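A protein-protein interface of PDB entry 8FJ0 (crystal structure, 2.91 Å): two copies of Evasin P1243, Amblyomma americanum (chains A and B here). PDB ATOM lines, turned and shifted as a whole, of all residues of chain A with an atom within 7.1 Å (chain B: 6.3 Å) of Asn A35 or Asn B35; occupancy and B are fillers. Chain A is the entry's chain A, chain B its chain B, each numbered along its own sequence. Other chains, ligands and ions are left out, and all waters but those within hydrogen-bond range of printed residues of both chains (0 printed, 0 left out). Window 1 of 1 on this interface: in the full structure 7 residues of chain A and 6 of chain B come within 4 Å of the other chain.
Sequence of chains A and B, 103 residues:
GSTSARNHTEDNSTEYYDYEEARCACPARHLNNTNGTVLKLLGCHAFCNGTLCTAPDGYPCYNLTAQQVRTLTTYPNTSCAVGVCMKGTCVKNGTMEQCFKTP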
ATOM      1  N   ASN A  32      13.321   2.936  17.583  1.00  0.00           N
ATOM      2  CA  ASN A  32      13.928   4.202  17.954  1.00  0.00           C
ATOM      3  C   ASN A  32      13.725   5.219  16.838  1.00  0.00           C
ATOM      4  O   ASN A  32      13.422   4.866  15.698  1.00  0.00           O
ATOM      5  CB  ASN A  32      15.418   4.020  18.243  1.00  0.00           C
ATOM      6  CG  ASN A  32      15.967   5.103  19.148  1.00  0.00           C
ATOM      7  OD1 ASN A  32      15.359   6.163  19.299  1.00  0.00           O
ATOM      8  ND2 ASN A  32      17.113   4.838  19.769  1.00  0.00           N
ATOM      9  N   ASN A  33      13.890   6.495  17.180  1.00  0.00           N
ATOM     10  CA  ASN A  33      13.666   7.575  16.230  1.00  0.00           C
ATOM     11  C   ASN A  33      14.674   8.691  16.462  1.00  0.00           C
ATOM     12  O   ASN A  33      14.937   9.074  17.607  1.00  0.00           O
ATOM     13  CB  ASN A  33      12.229   8.118  16.319  1.00  0.00           C
ATOM     14  CG  ASN A  33      11.919   8.752  17.661  1.00  0.00           C
ATOM     15  OD1 ASN A  33      12.263   9.907  17.909  1.00  0.00           O
ATOM     16  ND2 ASN A  33      11.261   7.999  18.534  1.00  0.00           N
ATOM     17  N   THR A  34      15.244   9.203  15.369  1.00  0.00           N
ATOM     18  CA  THR A  34      16.192  10.311  15.424  1.00  0.00           C
ATOM     19  C   THR A  34      15.535  11.644  15.757  1.00  0.00           C
ATOM     20  O   THR A  34      16.230  12.665  15.773  1.00  0.00           O
ATOM     21  CB  THR A  34      16.937  10.434  14.092  1.00  0.00           C
ATOM     22  OG1 THR A  34      16.167  11.232  13.185  1.00  0.00           O
ATOM     23  CG2 THR A  34      17.154   9.066  13.480  1.00  0.00           C
ATOM     24  N   ASN A  35      14.233  11.669  16.034  1.00  0.00           N
ATOM     25  CA  ASN A  35      13.528  12.906  16.325  1.00  0.00           C
ATOM     26  C   ASN A  35      13.412  13.185  17.815  1.00  0.00           C
ATOM     27  O   ASN A  35      12.815  14.196  18.191  1.00  0.00           O
ATOM     28  CB  ASN A  35      12.126  12.879  15.708  1.00  0.00           C
ATOM     29  CG  ASN A  35      12.151  12.675  14.206  1.00  0.00           C
ATOM     30  OD1 ASN A  35      12.225  11.544  13.722  1.00  0.00           O
ATOM     31  ND2 ASN A  35      12.092  13.773  13.458  1.00  0.00           N
ATOM     32  N   GLY A  36      13.929  12.308  18.667  1.00  0.00           N
ATOM     33  CA  GLY A  36      13.936  12.572  20.097  1.00  0.00           C
ATOM     34  C   GLY A  36      12.577  12.484  20.754  1.00  0.00           C
ATOM     35  O   GLY A  36      12.242  13.335  21.589  1.00  0.00           O
ATOM     36  N   THR A  37      11.791  11.470  20.415  1.00  0.00           N
ATOM     37  CA  THR A  37      10.458  11.275  20.969  1.00  0.00           C
ATOM     38  C   THR A  37      10.388   9.925  21.676  1.00  0.00           C
ATOM     39  O   THR A  37      11.355   9.159  21.704  1.00  0.00           O
ATOM     40  CB  THR A  37       9.387  11.369  19.878  1.00  0.00           C
ATOM     41  OG1 THR A  37       9.560  10.299  18.941  1.00  0.00           O
ATOM     42  CG2 THR A  37       9.475  12.704  19.150  1.00  0.00           C
ATOM     43  N   VAL A  38       9.232   9.655  22.281  1.00  0.00           N
ATOM     44  CA  VAL A  38       8.989   8.410  23.004  1.00  0.00           C
ATOM     45  C   VAL A  38       9.269   7.217  22.099  1.00  0.00           C
ATOM     46  O   VAL A  38       9.040   7.276  20.885  1.00  0.00           O
ATOM     47  CB  VAL A  38       7.553   8.358  23.556  1.00  0.00           C
ATOM     48  CG1 VAL A  38       7.356   9.429  24.611  1.00  0.00           C
ATOM     49  CG2 VAL A  38       6.539   8.532  22.435  1.00  0.00           C
ATOM     50  N   TYR A  62       4.231   2.467  15.800  1.00  0.00           N
ATOM     51  CA  TYR A  62       4.459   2.736  14.390  1.00  0.00           C
ATOM     52  C   TYR A  62       3.647   1.766  13.544  1.00  0.00           C
ATOM     53  O   TYR A  62       3.418   0.618  13.934  1.00  0.00           O
ATOM     54  CB  TYR A  62       5.939   2.617  14.020  1.00  0.00           C
ATOM     55  CG  TYR A  62       6.834   3.694  14.584  1.00  0.00           C
ATOM     56  CD1 TYR A  62       6.634   5.033  14.264  1.00  0.00           C
ATOM     57  CD2 TYR A  62       7.908   3.369  15.402  1.00  0.00           C
ATOM     58  CE1 TYR A  62       7.463   6.019  14.766  1.00  0.00           C
ATOM     59  CE2 TYR A  62       8.742   4.345  15.906  1.00  0.00           C
ATOM     60  CZ  TYR A  62       8.515   5.667  15.587  1.00  0.00           C
ATOM     61  OH  TYR A  62       9.350   6.637  16.093  1.00  0.00           O
ATOM     62  N   PRO A  76      18.072   5.981   9.845  1.00  0.00           N
ATOM     63  CA  PRO A  76      16.766   6.239   9.228  1.00  0.00           C
ATOM     64  C   PRO A  76      16.844   6.286   7.710  1.00  0.00           C
ATOM     65  O   PRO A  76      17.735   6.908   7.130  1.00  0.00           O
ATOM     66  CB  PRO A  76      16.369   7.598   9.809  1.00  0.00           C
ATOM     67  CG  PRO A  76      17.674   8.255  10.097  1.00  0.00           C
ATOM     68  CD  PRO A  76      18.557   7.148  10.601  1.00  0.00           C
ATOM     69  N   SER A  79      10.232   7.022   6.130  1.00  0.00           N
ATOM     70  CA  SER A  79       9.440   7.835   7.042  1.00  0.00           C
ATOM     71  C   SER A  79       8.361   6.940   7.638  1.00  0.00           C
ATOM     72  O   SER A  79       7.507   6.422   6.908  1.00  0.00           O
ATOM     73  CB  SER A  79       8.829   9.036   6.322  1.00  0.00           C
ATOM     74  N   CYS A  80       8.401   6.756   8.956  1.00  0.00           N
ATOM     75  CA  CYS A  80       7.538   5.814   9.651  1.00  0.00           C
ATOM     76  C   CYS A  80       6.311   6.540  10.178  1.00  0.00           C
ATOM     77  O   CYS A  80       6.416   7.643  10.726  1.00  0.00           O
ATOM     78  CB  CYS A  80       8.300   5.154  10.805  1.00  0.00           C
ATOM     79  SG  CYS A  80      10.037   4.755  10.383  1.00  0.00           S
ATOM     80  N   VAL A  82       3.516   7.369  12.581  1.00  0.00           N
ATOM     81  CA  VAL A  82       3.166   7.266  13.988  1.00  0.00           C
ATOM     82  C   VAL A  82       1.675   6.976  14.124  1.00  0.00           C
ATOM     83  O   VAL A  82       0.860   7.360  13.273  1.00  0.00           O
ATOM     84  CB  VAL A  82       3.567   8.559  14.721  1.00  0.00           C
ATOM     85  CG1 VAL A  82       3.113   8.547  16.167  1.00  0.00           C
ATOM     86  CG2 VAL A  82       5.072   8.754  14.643  1.00  0.00           C
ATOM     87  N   GLY A  94      -1.342  10.943  11.282  1.00  0.00           N
ATOM     88  CA  GLY A  94      -0.750  11.950  10.423  1.00  0.00           C
ATOM     89  C   GLY A  94       0.729  12.196  10.621  1.00  0.00           C
ATOM     90  O   GLY A  94       1.443  12.477   9.656  1.00  0.00           O
ATOM     91  N   THR A  95       1.200  12.108  11.865  1.00  0.00           N
ATOM     92  CA  THR A  95       2.579  12.453  12.183  1.00  0.00           C
ATOM     93  C   THR A  95       3.535  11.396  11.643  1.00  0.00           C
ATOM     94  O   THR A  95       3.199  10.214  11.538  1.00  0.00           O
ATOM     95  CB  THR A  95       2.765  12.602  13.693  1.00  0.00           C
ATOM     96  OG1 THR A  95       2.246  11.446  14.358  1.00  0.00           O
ATOM     97  CG2 THR A  95       2.044  13.840  14.204  1.00  0.00           C
ATOM     98  N   MET A  96       4.745  11.830  11.308  1.00  0.00           N
ATOM     99  CA  MET A  96       5.757  10.935  10.774  1.00  0.00           C
ATOM    100  C   MET A  96       7.070  11.136  11.517  1.00  0.00           C
ATOM    101  O   MET A  96       7.356  12.227  12.020  1.00  0.00           O
ATOM    102  CB  MET A  96       5.967  11.182   9.273  1.00  0.00           C
ATOM    103  CG  MET A  96       4.687  11.197   8.440  1.00  0.00           C
ATOM    104  SD  MET A  96       4.125   9.588   7.846  1.00  0.00           S
ATOM    105  CE  MET A  96       5.227   9.325   6.458  1.00  0.00           C
ATOM    106  N   GLU A  97       7.863  10.067  11.598  1.00  0.00           N
ATOM    107  CA  GLU A  97       9.145  10.122  12.287  1.00  0.00           C
ATOM    108  C   GLU A  97      10.178   9.303  11.528  1.00  0.00           C
ATOM    109  O   GLU A  97       9.854   8.303  10.886  1.00  0.00           O
ATOM    110  CB  GLU A  97       9.036   9.616  13.736  1.00  0.00           C
ATOM    111  CG  GLU A  97       8.470  10.635  14.717  1.00  0.00           C
ATOM    112  CD  GLU A  97       8.074  10.014  16.046  1.00  0.00           C
ATOM    113  OE1 GLU A  97       8.398   8.828  16.279  1.00  0.00           O
ATOM    114  OE2 GLU A  97       7.426  10.712  16.859  1.00  0.00           O
ATOM    115  N   GLN A  98      11.426   9.754  11.582  1.00  0.00           N
ATOM    116  CA  GLN A  98      12.536   8.973  11.047  1.00  0.00           C
ATOM    117  C   GLN A  98      12.907   7.911  12.075  1.00  0.00           C
ATOM    118  O   GLN A  98      13.491   8.225  13.117  1.00  0.00           O
ATOM    119  CB  GLN A  98      13.723   9.875  10.717  1.00  0.00           C
ATOM    120  CG  GLN A  98      13.554  10.710   9.452  1.00  0.00           C
ATOM    121  CD  GLN A  98      12.415  11.710   9.541  1.00  0.00           C
ATOM    122  OE1 GLN A  98      12.528  12.744  10.201  1.00  0.00           O
ATOM    123  NE2 GLN A  98      11.309  11.404   8.873  1.00  0.00           N
ATOM    124  N   CYS A  99      12.584   6.654  11.791  1.00  0.00           N
ATOM    125  CA  CYS A  99      12.737   5.588  12.766  1.00  0.00           C
ATOM    126  C   CYS A  99      13.665   4.511  12.224  1.00  0.00           C
ATOM    127  O   CYS A  99      13.768   4.304  11.010  1.00  0.00           O
ATOM    128  CB  CYS A  99      11.381   4.970  13.136  1.00  0.00           C
ATOM    129  SG  CYS A  99      10.763   3.720  11.979  1.00  0.00           S
ATOM    130  N   PHE A 100      14.338   3.823  13.144  1.00  0.00           N
ATOM    131  CA  PHE A 100      15.387   2.885  12.775  1.00  0.00           C
ATOM    132  C   PHE A 100      15.408   1.737  13.770  1.00  0.00           C
ATOM    133  O   PHE A 100      14.865   1.831  14.875  1.00  0.00           O
ATOM    134  CB  PHE A 100      16.759   3.567  12.710  1.00  0.00           C
ATOM    135  CG  PHE A 100      17.167   4.236  13.989  1.00  0.00           C
ATOM    136  CD1 PHE A 100      16.712   5.508  14.299  1.00  0.00           C
ATOM    137  CD2 PHE A 100      18.017   3.597  14.878  1.00  0.00           C
ATOM    138  CE1 PHE A 100      17.090   6.124  15.476  1.00  0.00           C
ATOM    139  CE2 PHE A 100      18.404   4.206  16.057  1.00  0.00           C
ATOM    140  CZ  PHE A 100      17.942   5.472  16.354  1.00  0.00           C
ATOM    141  N   ASN B  33       7.666  21.158   7.572  1.00  0.00           N
ATOM    142  CA  ASN B  33       8.280  19.923   8.039  1.00  0.00           C
ATOM    143  C   ASN B  33       7.555  18.730   7.434  1.00  0.00           C
ATOM    144  O   ASN B  33       6.321  18.696   7.403  1.00  0.00           O
ATOM    145  CB  ASN B  33       8.267  19.841   9.574  1.00  0.00           C
ATOM    146  CG  ASN B  33       6.858  19.792  10.151  1.00  0.00           C
ATOM    147  OD1 ASN B  33       6.223  18.740  10.184  1.00  0.00           O
ATOM    148  ND2 ASN B  33       6.370  20.933  10.616  1.00  0.00           N
ATOM    149  N   THR B  34       8.329  17.766   6.932  1.00  0.00           N
ATOM    150  CA  THR B  34       7.782  16.538   6.363  1.00  0.00           C
ATOM    151  C   THR B  34       7.243  15.575   7.414  1.00  0.00           C
ATOM    152  O   THR B  34       6.820  14.470   7.052  1.00  0.00           O
ATOM    153  CB  THR B  34       8.845  15.832   5.520  1.00  0.00           C
ATOM    154  N   ASN B  35       7.239  15.952   8.690  1.00  0.00           N
ATOM    155  CA  ASN B  35       6.780  15.073   9.754  1.00  0.00           C
ATOM    156  C   ASN B  35       5.329  15.320  10.141  1.00  0.00           C
ATOM    157  O   ASN B  35       4.813  14.626  11.022  1.00  0.00           O
ATOM    158  CB  ASN B  35       7.673  15.236  10.989  1.00  0.00           C
ATOM    159  CG  ASN B  35       9.132  14.969  10.691  1.00  0.00           C
ATOM    160  OD1 ASN B  35       9.845  15.850  10.219  1.00  0.00           O
ATOM    161  ND2 ASN B  35       9.587  13.753  10.970  1.00  0.00           N
ATOM    162  N   GLY B  36       4.663  16.285   9.517  1.00  0.00           N
ATOM    163  CA  GLY B  36       3.256  16.511   9.796  1.00  0.00           C
ATOM    164  C   GLY B  36       3.005  17.127  11.156  1.00  0.00           C
ATOM    165  O   GLY B  36       2.088  16.699  11.868  1.00  0.00           O
ATOM    166  N   THR B  37       3.792  18.126  11.531  1.00  0.00           N
ATOM    167  CA  THR B  37       3.676  18.797  12.816  1.00  0.00           C
ATOM    168  C   THR B  37       3.398  20.281  12.597  1.00  0.00           C
ATOM    169  O   THR B  37       3.337  20.766  11.464  1.00  0.00           O
ATOM    170  CB  THR B  37       4.942  18.595  13.654  1.00  0.00           C
ATOM    171  N   GLY B  94      15.155  18.484  22.983  1.00  0.00           N
ATOM    172  CA  GLY B  94      15.552  17.216  22.397  1.00  0.00           C
ATOM    173  C   GLY B  94      15.096  16.927  20.980  1.00  0.00           C
ATOM    174  O   GLY B  94      15.823  16.293  20.209  1.00  0.00           O
ATOM    175  N   THR B  95      13.906  17.397  20.617  1.00  0.00           N
ATOM    176  CA  THR B  95      13.288  16.998  19.362  1.00  0.00           C
ATOM    177  C   THR B  95      13.977  17.604  18.140  1.00  0.00           C
ATOM    178  O   THR B  95      14.499  18.722  18.170  1.00  0.00           O
ATOM    179  CB  THR B  95      11.808  17.384  19.367  1.00  0.00           C
ATOM    180  OG1 THR B  95      11.672  18.764  19.729  1.00  0.00           O
ATOM    181  CG2 THR B  95      11.045  16.527  20.367  1.00  0.00           C
ATOM    182  N   MET B  96      13.966  16.832  17.052  1.00  0.00           N
ATOM    183  CA  MET B  96      14.484  17.226  15.750  1.00  0.00           C
ATOM    184  C   MET B  96      13.464  16.829  14.694  1.00  0.00           C
ATOM    185  O   MET B  96      12.706  15.873  14.879  1.00  0.00           O
ATOM    186  CB  MET B  96      15.837  16.567  15.439  1.00  0.00           C
ATOM    187  CG  MET B  96      16.908  16.754  16.499  1.00  0.00           C
ATOM    188  SD  MET B  96      17.840  18.277  16.257  1.00  0.00           S
ATOM    189  CE  MET B  96      18.798  18.352  17.770  1.00  0.00           C
ATOM    190  N   GLU B  97      13.434  17.573  13.590  1.00  0.00           N
ATOM    191  CA  GLU B  97      12.485  17.282  12.521  1.00  0.00           C
ATOM    192  C   GLU B  97      13.142  17.484  11.165  1.00  0.00           C
ATOM    193  O   GLU B  97      14.003  18.346  10.999  1.00  0.00           O
ATOM    194  CB  GLU B  97      11.229  18.163  12.603  1.00  0.00           C
ATOM    195  CG  GLU B  97      10.584  18.222  13.973  1.00  0.00           C
ATOM    196  CD  GLU B  97       9.072  18.177  13.923  1.00  0.00           C
ATOM    197  OE1 GLU B  97       8.526  17.156  13.452  1.00  0.00           O
ATOM    198  OE2 GLU B  97       8.427  19.155  14.362  1.00  0.00           O
ATOM    199  N   GLN B  98      12.726  16.683  10.190  1.00  0.00           N
ATOM    200  CA  GLN B  98      13.157  16.902   8.813  1.00  0.00           C
ATOM    201  C   GLN B  98      12.338  18.054   8.247  1.00  0.00           C
ATOM    202  O   GLN B  98      11.149  17.896   7.956  1.00  0.00           O
ATOM    203  CB  GLN B  98      12.983  15.636   7.982  1.00  0.00           C
ATOM    204  N   CYS B  99      12.969  19.213   8.079  1.00  0.00           N
ATOM    205  CA  CYS B  99      12.257  20.431   7.726  1.00  0.00           C
ATOM    206  C   CYS B  99      12.801  20.995   6.421  1.00  0.00           C
ATOM    207  O   CYS B  99      13.969  20.801   6.078  1.00  0.00           O
ATOM    208  CB  CYS B  99      12.368  21.491   8.838  1.00  0.00           C
ATOM    209  SG  CYS B  99      13.872  22.517   8.833  1.00  0.00           S
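O of Asn B35 is in hydrogen-bond range of N of Met A96, 2.8 Å away. OE1 of Gln A98 lies within hydrogen-bond range of ND2 of Asn B35, at 3.2 Å. The backbone carbonyl oxygen of Met B96 sits at hydrogen-bond distance from the side-chain amide nitrogen of Asn A35 (2.6 Å).
Along chain B the printed residues that touch a printed residue of chain A span positions 35 to 98. Printed residues of chain A that touch a printed residue of chain B: Thr A34, Asn A35, Gly A36, Thr A95, Met A96, Glu A97 and Gln A98. Among the printed residues, 12 pairs touch across the chains.
Met B96 touches Thr A34 (CB to O, 3.9 Å). Asn A35 touches Asn B35. CA of Thr B95 touches O of Asn A35 (3.1 Å). CA of Glu B97 touches ND2 of Asn A35 (3.7 Å). CG2 of Thr B95 touches O of Gly A36, 3.6 Å away. Thr A95 touches Asn B35 (CA to O, 3.3 Å). CG2 of Thr A95 touches O of Gly B36 (3.7 Å). CA of Glu A97 touches ND2 of Asn B35 (3.9 Å). Gln B98 touches Gln A98 (CB to OE1, 3.7 Å).
N of Cys A80 sits at hydrogen-bond distance from O of Glu A97 (2.9 Å). The side-chain amide oxygen of Asn A33 sits at hydrogen-bond distance from the backbone NH of Gly A36 (3.0 Å). The side-chain amide oxygen of Asn A35 sits at hydrogen-bond distance from the backbone NH of Gln A98, 2.9 Å away. SG of Cys A99 is disulfide-bonded to SG of Cys A80 (2.0 Å). The backbone NH of Asn B35 lies close to the side-chain amide oxygen of Asn B33. The backbone carbonyl oxygen (O) of Gln B98 sits at hydrogen-bond distance from the backbone NH (N) of Thr B34 (3.0 Å).
Of chain B, only Asn B35, Thr B95, Met B96 and Glu B97 come within 4 Å of Asn A35. Tyr A62 touches none of the printed residues of chain B. Printed residues of chain B within 4 Å of Gln A98: Asn B35 (3.2 Å) and Gln B98 (3.7 Å). Of chain A, only Asn A35, Thr A95, Met A96, Glu A97 and Gln A98 come within 4 Å of Asn B35. Of the printed residues of chain A, Gly B36 touches Thr A95 (3.7 Å). The nearest residue of chain B that does not touch Asn A35 is Gly B94 (4.2 Å). The nearest residue of chain A that does not touch Asn B35 is Gly A94 (4.2 Å). The nearest printed residue of chain B that does not touch Gly A36 is Gly B94 (4.2 Å).
Thr A34 touches Met B96, but with the chains exchanged Met A96 does not touch Thr B34 (4.1 Å). Asn B35 touches its own counterpart, Asn A35. Asn A35 touches Met B96, and with the chains exchanged Met A96 touches Asn B35. Asn A35 touches Glu B97, and with the chains exchanged Glu A97 touches Asn B35. Positions printed for both chains: 33, 34, 35, 36, 37, 94, 95, 96, 97, 98 and 99. Of the 12 pairs that touch across the chains among the printed residues, 10 have their exchanged pair printed and touching as well.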
